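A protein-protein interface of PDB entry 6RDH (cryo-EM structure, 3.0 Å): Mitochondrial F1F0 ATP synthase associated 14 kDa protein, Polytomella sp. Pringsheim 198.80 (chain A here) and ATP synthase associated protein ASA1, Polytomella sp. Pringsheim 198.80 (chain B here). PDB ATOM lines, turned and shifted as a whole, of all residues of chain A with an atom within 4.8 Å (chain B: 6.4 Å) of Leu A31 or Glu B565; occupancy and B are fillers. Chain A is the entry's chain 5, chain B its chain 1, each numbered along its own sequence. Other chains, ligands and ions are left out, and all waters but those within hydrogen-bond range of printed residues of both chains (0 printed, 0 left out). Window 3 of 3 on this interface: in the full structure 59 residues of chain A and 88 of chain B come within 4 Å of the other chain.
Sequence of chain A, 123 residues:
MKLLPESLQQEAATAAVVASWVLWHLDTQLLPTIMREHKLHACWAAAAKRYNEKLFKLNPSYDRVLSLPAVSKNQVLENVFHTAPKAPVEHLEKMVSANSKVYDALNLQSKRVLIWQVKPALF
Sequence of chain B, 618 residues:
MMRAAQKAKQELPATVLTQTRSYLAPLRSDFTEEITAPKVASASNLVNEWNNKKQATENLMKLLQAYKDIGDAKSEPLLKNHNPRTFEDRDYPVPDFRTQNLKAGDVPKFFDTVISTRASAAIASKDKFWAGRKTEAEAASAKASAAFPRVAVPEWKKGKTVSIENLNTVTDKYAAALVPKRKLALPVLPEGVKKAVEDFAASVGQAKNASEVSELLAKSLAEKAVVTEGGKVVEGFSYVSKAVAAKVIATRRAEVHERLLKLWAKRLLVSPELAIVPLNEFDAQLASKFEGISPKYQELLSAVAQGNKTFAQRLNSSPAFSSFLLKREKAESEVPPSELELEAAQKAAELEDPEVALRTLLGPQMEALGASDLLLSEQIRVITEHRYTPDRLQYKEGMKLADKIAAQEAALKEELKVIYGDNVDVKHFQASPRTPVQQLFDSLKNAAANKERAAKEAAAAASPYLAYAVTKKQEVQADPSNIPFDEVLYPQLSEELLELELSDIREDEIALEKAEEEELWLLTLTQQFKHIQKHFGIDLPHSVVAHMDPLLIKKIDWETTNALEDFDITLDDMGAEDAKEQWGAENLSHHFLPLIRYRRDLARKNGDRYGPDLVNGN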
ATOM      1  N   LEU A  26     -15.160 -21.502   0.083  1.00  0.00           N
ATOM      2  CA  LEU A  26     -15.337 -21.066  -1.292  1.00  0.00           C
ATOM      3  C   LEU A  26     -15.486 -22.254  -2.223  1.00  0.00           C
ATOM      4  O   LEU A  26     -16.591 -22.545  -2.686  1.00  0.00           O
ATOM      5  CB  LEU A  26     -14.134 -20.237  -1.687  1.00  0.00           C
ATOM      6  CG  LEU A  26     -14.102 -19.570  -3.029  1.00  0.00           C
ATOM      7  CD1 LEU A  26     -15.066 -18.429  -3.050  1.00  0.00           C
ATOM      8  CD2 LEU A  26     -12.720 -19.109  -3.176  1.00  0.00           C
ATOM      9  N   ASP A  27     -14.423 -23.046  -2.340  1.00  0.00           N
ATOM     10  CA  ASP A  27     -14.301 -24.128  -3.300  1.00  0.00           C
ATOM     11  C   ASP A  27     -15.327 -25.230  -3.122  1.00  0.00           C
ATOM     12  O   ASP A  27     -15.624 -25.941  -4.081  1.00  0.00           O
ATOM     13  CB  ASP A  27     -12.916 -24.706  -3.149  1.00  0.00           C
ATOM     14  CG  ASP A  27     -12.328 -25.120  -4.434  1.00  0.00           C
ATOM     15  OD1 ASP A  27     -13.003 -24.965  -5.467  1.00  0.00           O
ATOM     16  OD2 ASP A  27     -11.176 -25.581  -4.411  1.00  0.00           O
ATOM     17  N   GLN A  29     -18.499 -24.983  -0.710  1.00  0.00           N
ATOM     18  CA  GLN A  29     -19.865 -24.572  -0.485  1.00  0.00           C
ATOM     19  C   GLN A  29     -20.301 -23.416  -1.359  1.00  0.00           C
ATOM     20  O   GLN A  29     -21.475 -23.364  -1.727  1.00  0.00           O
ATOM     21  CB  GLN A  29     -20.049 -24.195   0.978  1.00  0.00           C
ATOM     22  CG  GLN A  29     -19.418 -25.168   1.924  1.00  0.00           C
ATOM     23  CD  GLN A  29     -20.240 -26.400   2.102  1.00  0.00           C
ATOM     24  OE1 GLN A  29     -19.719 -27.468   2.389  1.00  0.00           O
ATOM     25  NE2 GLN A  29     -21.542 -26.266   1.932  1.00  0.00           N
ATOM     26  N   LEU A  30     -19.415 -22.485  -1.708  1.00  0.00           N
ATOM     27  CA  LEU A  30     -19.893 -21.331  -2.449  1.00  0.00           C
ATOM     28  C   LEU A  30     -19.773 -21.538  -3.946  1.00  0.00           C
ATOM     29  O   LEU A  30     -20.743 -21.322  -4.663  1.00  0.00           O
ATOM     30  CB  LEU A  30     -19.134 -20.076  -2.032  1.00  0.00           C
ATOM     31  CG  LEU A  30     -19.379 -19.546  -0.629  1.00  0.00           C
ATOM     32  CD1 LEU A  30     -18.467 -18.390  -0.379  1.00  0.00           C
ATOM     33  CD2 LEU A  30     -20.804 -19.120  -0.473  1.00  0.00           C
ATOM     34  N   LEU A  31     -18.611 -21.979  -4.425  1.00  0.00           N
ATOM     35  CA  LEU A  31     -18.402 -22.108  -5.863  1.00  0.00           C
ATOM     36  C   LEU A  31     -19.270 -23.152  -6.564  1.00  0.00           C
ATOM     37  O   LEU A  31     -19.594 -22.919  -7.740  1.00  0.00           O
ATOM     38  CB  LEU A  31     -16.919 -22.376  -6.148  1.00  0.00           C
ATOM     39  CG  LEU A  31     -16.074 -21.223  -6.667  1.00  0.00           C
ATOM     40  CD1 LEU A  31     -14.719 -21.737  -7.059  1.00  0.00           C
ATOM     41  CD2 LEU A  31     -16.762 -20.601  -7.838  1.00  0.00           C
ATOM     42  N   PRO A  32     -19.660 -24.287  -5.967  1.00  0.00           N
ATOM     43  CA  PRO A  32     -20.755 -25.055  -6.573  1.00  0.00           C
ATOM     44  C   PRO A  32     -22.060 -24.300  -6.676  1.00  0.00           C
ATOM     45  O   PRO A  32     -22.737 -24.394  -7.700  1.00  0.00           O
ATOM     46  CB  PRO A  32     -20.870 -26.248  -5.634  1.00  0.00           C
ATOM     47  CG  PRO A  32     -19.515 -26.494  -5.283  1.00  0.00           C
ATOM     48  CD  PRO A  32     -18.903 -25.164  -5.060  1.00  0.00           C
ATOM     49  N   THR A  33     -22.415 -23.523  -5.663  1.00  0.00           N
ATOM     50  CA  THR A  33     -23.659 -22.768  -5.692  1.00  0.00           C
ATOM     51  C   THR A  33     -23.582 -21.594  -6.658  1.00  0.00           C
ATOM     52  O   THR A  33     -24.574 -21.267  -7.312  1.00  0.00           O
ATOM     53  CB  THR A  33     -23.975 -22.293  -4.286  1.00  0.00           C
ATOM     54  OG1 THR A  33     -23.874 -23.404  -3.393  1.00  0.00           O
ATOM     55  CG2 THR A  33     -25.339 -21.748  -4.215  1.00  0.00           C
ATOM     56  N   ILE A  34     -22.420 -20.937  -6.738  1.00  0.00           N
ATOM     57  CA  ILE A  34     -22.181 -19.925  -7.764  1.00  0.00           C
ATOM     58  C   ILE A  34     -22.347 -20.539  -9.140  1.00  0.00           C
ATOM     59  O   ILE A  34     -23.073 -20.017  -9.988  1.00  0.00           O
ATOM     60  CB  ILE A  34     -20.771 -19.318  -7.628  1.00  0.00           C
ATOM     61  CG1 ILE A  34     -20.529 -18.616  -6.300  1.00  0.00           C
ATOM     62  CG2 ILE A  34     -20.504 -18.356  -8.742  1.00  0.00           C
ATOM     63  CD1 ILE A  34     -21.399 -17.514  -6.020  1.00  0.00           C
ATOM     64  N   MET A  35     -21.703 -21.681  -9.366  1.00  0.00           N
ATOM     65  CA  MET A  35     -21.585 -22.212 -10.711  1.00  0.00           C
ATOM     66  C   MET A  35     -22.841 -22.912 -11.181  1.00  0.00           C
ATOM     67  O   MET A  35     -23.070 -22.965 -12.382  1.00  0.00           O
ATOM     68  CB  MET A  35     -20.399 -23.161 -10.797  1.00  0.00           C
ATOM     69  CG  MET A  35     -19.092 -22.450 -10.973  1.00  0.00           C
ATOM     70  SD  MET A  35     -19.273 -21.022 -12.034  1.00  0.00           S
ATOM     71  CE  MET A  35     -17.924 -20.036 -11.455  1.00  0.00           C
ATOM     72  N   LYS A  39     -24.114 -21.374 -14.499  1.00  0.00           N
ATOM     73  CA  LYS A  39     -24.013 -22.185 -15.688  1.00  0.00           C
ATOM     74  C   LYS A  39     -25.343 -22.713 -16.176  1.00  0.00           C
ATOM     75  O   LYS A  39     -25.416 -23.069 -17.342  1.00  0.00           O
ATOM     76  CB  LYS A  39     -23.055 -23.336 -15.456  1.00  0.00           C
ATOM     77  CG  LYS A  39     -21.653 -22.881 -15.403  1.00  0.00           C
ATOM     78  CD  LYS A  39     -20.715 -24.017 -15.407  1.00  0.00           C
ATOM     79  CE  LYS A  39     -19.332 -23.511 -15.240  1.00  0.00           C
ATOM     80  NZ  LYS A  39     -18.408 -24.630 -15.099  1.00  0.00           N
ATOM     81  N   GLU B 559     -18.152 -30.196 -14.013  1.00  0.00           N
ATOM     82  CA  GLU B 559     -17.237 -29.096 -14.307  1.00  0.00           C
ATOM     83  C   GLU B 559     -16.641 -28.504 -13.041  1.00  0.00           C
ATOM     84  O   GLU B 559     -15.497 -28.048 -13.046  1.00  0.00           O
ATOM     85  CB  GLU B 559     -17.946 -28.001 -15.077  1.00  0.00           C
ATOM     86  CG  GLU B 559     -18.435 -28.427 -16.393  1.00  0.00           C
ATOM     87  CD  GLU B 559     -18.720 -27.275 -17.297  1.00  0.00           C
ATOM     88  OE1 GLU B 559     -18.349 -26.148 -16.940  1.00  0.00           O
ATOM     89  OE2 GLU B 559     -19.312 -27.488 -18.366  1.00  0.00           O
ATOM     90  N   THR B 560     -17.404 -28.474 -11.955  1.00  0.00           N
ATOM     91  CA  THR B 560     -16.851 -27.984 -10.696  1.00  0.00           C
ATOM     92  C   THR B 560     -15.886 -28.994 -10.087  1.00  0.00           C
ATOM     93  O   THR B 560     -14.834 -28.614  -9.570  1.00  0.00           O
ATOM     94  CB  THR B 560     -17.975 -27.653  -9.723  1.00  0.00           C
ATOM     95  OG1 THR B 560     -18.881 -26.736 -10.337  1.00  0.00           O
ATOM     96  CG2 THR B 560     -17.438 -27.016  -8.497  1.00  0.00           C
ATOM     97  N   THR B 561     -16.214 -30.285 -10.166  1.00  0.00           N
ATOM     98  CA  THR B 561     -15.371 -31.331  -9.595  1.00  0.00           C
ATOM     99  C   THR B 561     -14.043 -31.435 -10.321  1.00  0.00           C
ATOM    100  O   THR B 561     -13.000 -31.654  -9.698  1.00  0.00           O
ATOM    101  CB  THR B 561     -16.095 -32.674  -9.657  1.00  0.00           C
ATOM    102  OG1 THR B 561     -17.433 -32.517  -9.189  1.00  0.00           O
ATOM    103  CG2 THR B 561     -15.417 -33.686  -8.795  1.00  0.00           C
ATOM    104  N   ASN B 562     -14.057 -31.275 -11.638  1.00  0.00           N
ATOM    105  CA  ASN B 562     -12.872 -31.476 -12.454  1.00  0.00           C
ATOM    106  C   ASN B 562     -12.204 -30.173 -12.839  1.00  0.00           C
ATOM    107  O   ASN B 562     -11.695 -30.056 -13.955  1.00  0.00           O
ATOM    108  CB  ASN B 562     -13.228 -32.282 -13.688  1.00  0.00           C
ATOM    109  CG  ASN B 562     -13.695 -33.655 -13.338  1.00  0.00           C
ATOM    110  OD1 ASN B 562     -14.450 -33.839 -12.400  1.00  0.00           O
ATOM    111  ND2 ASN B 562     -13.214 -34.638 -14.061  1.00  0.00           N
ATOM    112  N   ALA B 563     -12.239 -29.185 -11.942  1.00  0.00           N
ATOM    113  CA  ALA B 563     -11.453 -27.955 -11.992  1.00  0.00           C
ATOM    114  C   ALA B 563     -11.738 -27.105 -13.214  1.00  0.00           C
ATOM    115  O   ALA B 563     -10.905 -26.290 -13.607  1.00  0.00           O
ATOM    116  CB  ALA B 563      -9.957 -28.252 -11.906  1.00  0.00           C
ATOM    117  N   LEU B 564     -12.896 -27.269 -13.826  1.00  0.00           N
ATOM    118  CA  LEU B 564     -13.267 -26.528 -15.017  1.00  0.00           C
ATOM    119  C   LEU B 564     -14.432 -25.607 -14.720  1.00  0.00           C
ATOM    120  O   LEU B 564     -15.304 -25.393 -15.550  1.00  0.00           O
ATOM    121  CB  LEU B 564     -13.610 -27.473 -16.158  1.00  0.00           C
ATOM    122  CG  LEU B 564     -12.468 -28.308 -16.708  1.00  0.00           C
ATOM    123  CD1 LEU B 564     -13.036 -29.389 -17.581  1.00  0.00           C
ATOM    124  CD2 LEU B 564     -11.537 -27.429 -17.492  1.00  0.00           C
ATOM    125  N   GLU B 565     -14.443 -25.044 -13.518  1.00  0.00           N
ATOM    126  CA  GLU B 565     -15.511 -24.156 -13.094  1.00  0.00           C
ATOM    127  C   GLU B 565     -15.488 -22.833 -13.830  1.00  0.00           C
ATOM    128  O   GLU B 565     -16.489 -22.118 -13.830  1.00  0.00           O
ATOM    129  CB  GLU B 565     -15.370 -23.937 -11.603  1.00  0.00           C
ATOM    130  CG  GLU B 565     -13.977 -23.540 -11.264  1.00  0.00           C
ATOM    131  CD  GLU B 565     -13.504 -24.144  -9.986  1.00  0.00           C
ATOM    132  OE1 GLU B 565     -14.322 -24.780  -9.296  1.00  0.00           O
ATOM    133  OE2 GLU B 565     -12.298 -24.023  -9.691  1.00  0.00           O
ATOM    134  N   ASP B 566     -14.372 -22.492 -14.449  1.00  0.00           N
ATOM    135  CA  ASP B 566     -14.256 -21.310 -15.278  1.00  0.00           C
ATOM    136  C   ASP B 566     -14.158 -21.674 -16.750  1.00  0.00           C
ATOM    137  O   ASP B 566     -13.469 -20.995 -17.507  1.00  0.00           O
ATOM    138  CB  ASP B 566     -13.038 -20.500 -14.857  1.00  0.00           C
ATOM    139  CG  ASP B 566     -11.760 -21.309 -14.896  1.00  0.00           C
ATOM    140  OD1 ASP B 566     -11.757 -22.465 -14.445  1.00  0.00           O
ATOM    141  OD2 ASP B 566     -10.745 -20.785 -15.384  1.00  0.00           O
ATOM    142  N   PHE B 567     -14.835 -22.745 -17.169  1.00  0.00           N
ATOM    143  CA  PHE B 567     -14.620 -23.233 -18.524  1.00  0.00           C
ATOM    144  C   PHE B 567     -15.287 -22.344 -19.554  1.00  0.00           C
ATOM    145  O   PHE B 567     -14.745 -22.159 -20.644  1.00  0.00           O
ATOM    146  CB  PHE B 567     -15.104 -24.664 -18.689  1.00  0.00           C
ATOM    147  CG  PHE B 567     -14.715 -25.266 -19.999  1.00  0.00           C
ATOM    148  CD1 PHE B 567     -13.387 -25.328 -20.367  1.00  0.00           C
ATOM    149  CD2 PHE B 567     -15.669 -25.744 -20.871  1.00  0.00           C
ATOM    150  CE1 PHE B 567     -13.018 -25.862 -21.572  1.00  0.00           C
ATOM    151  CE2 PHE B 567     -15.305 -26.275 -22.079  1.00  0.00           C
ATOM    152  CZ  PHE B 567     -13.980 -26.336 -22.429  1.00  0.00           C
ATOM    153  N   ASP B 568     -16.448 -21.772 -19.244  1.00  0.00           N
ATOM    154  CA  ASP B 568     -16.997 -20.803 -20.181  1.00  0.00           C
ATOM    155  C   ASP B 568     -16.205 -19.505 -20.163  1.00  0.00           C
ATOM    156  O   ASP B 568     -16.087 -18.844 -21.200  1.00  0.00           O
ATOM    157  CB  ASP B 568     -18.468 -20.540 -19.901  1.00  0.00           C
ATOM    158  CG  ASP B 568     -18.724 -20.074 -18.505  1.00  0.00           C
ATOM    159  OD1 ASP B 568     -18.189 -20.686 -17.566  1.00  0.00           O
ATOM    160  OD2 ASP B 568     -19.480 -19.101 -18.345  1.00  0.00           O
ATOM    161  N   ILE B 569     -15.628 -19.149 -19.013  1.00  0.00           N
ATOM    162  CA  ILE B 569     -14.740 -17.997 -18.949  1.00  0.00           C
ATOM    163  C   ILE B 569     -13.474 -18.266 -19.732  1.00  0.00           C
ATOM    164  O   ILE B 569     -12.938 -17.363 -20.376  1.00  0.00           O
ATOM    165  CB  ILE B 569     -14.423 -17.626 -17.494  1.00  0.00           C
ATOM    166  CG1 ILE B 569     -15.661 -17.774 -16.626  1.00  0.00           C
ATOM    167  CG2 ILE B 569     -13.956 -16.208 -17.414  1.00  0.00           C
ATOM    168  CD1 ILE B 569     -15.399 -17.548 -15.170  1.00  0.00           C
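The side-chain sulfur (SD) of Met A35 lies close to the backbone carbonyl oxygen (O) of Glu B565 (3.5 Å).
O of Glu B565 lies within hydrogen-bond range of NZ of Lys A39.
The side-chain amino group (NZ) of Lys A39 sits close to the side-chain carboxylate (OE1) of Glu B559, at 2.4 Å.
The side-chain amino group (NZ) of Lys A39 sits at hydrogen-bond distance from the backbone carbonyl oxygen (O) of Leu B564, at 3.2 Å.
Of the 11 printed residues of chain B, 5 touch a printed residue of chain A.
Of the 10 printed residues of chain A, 4 touch a printed residue of chain B.
Hydrophobic or aromatic side chains of chain A that line the printed part of chain B: Leu A31, Pro A32 and Met A35.
Along chain A the printed residues that touch a printed residue of chain B span positions 31 to 39.
Among the printed residues, Asp or Glu carboxylates within 4 Å of a Lys or Arg side-chain nitrogen of the other chain: Lys A39 with Glu B559 (2.4 Å).
O of Glu B559 sits at hydrogen-bond distance from N of Glu B565 (3.2 Å).
O of Leu A26 sits at hydrogen-bond distance from N of Leu A31 (2.7 Å).
N of Leu B564 sits at hydrogen-bond distance from O of Glu B559 (2.8 Å).
Among the printed residues, pairs that only touch across the chains: Leu A31 with Glu B565, Lys A39 with Asp B568, Pro A32 with Thr B560 and Met A35 with Thr B560.
Of chain B, only Glu B565 comes within 4 Å of Leu A31.
Of the printed residues of chain A, Leu B564 touches Lys A39 (3.2 Å).
Printed residues of chain A within 4 Å of Thr B560: Pro A32 and Met A35.
Printed residues of chain B within 4 Å of Met A35: Thr B560 (3.9 Å) and Glu B565 (3.5 Å).
Of the printed residues of chain B, Lys A39 touches Glu B559 (2.4 Å), Leu B564 (3.2 Å), Glu B565 (3.4 Å) and Asp B568 (3.8 Å).
Printed residues of chain A within 4 Å of Asp B568: Lys A39.
Phe B567 touches none of the printed residues of chain A.
The nearest residue of chain B that does not touch Leu A31 is Thr B560 (4.7 Å).
The nearest residue of chain A that does not touch Glu B565 is Asp A27 (4.1 Å).
The nearest printed residue of chain A that does not touch Glu B559 is Met A35 (6.9 Å).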
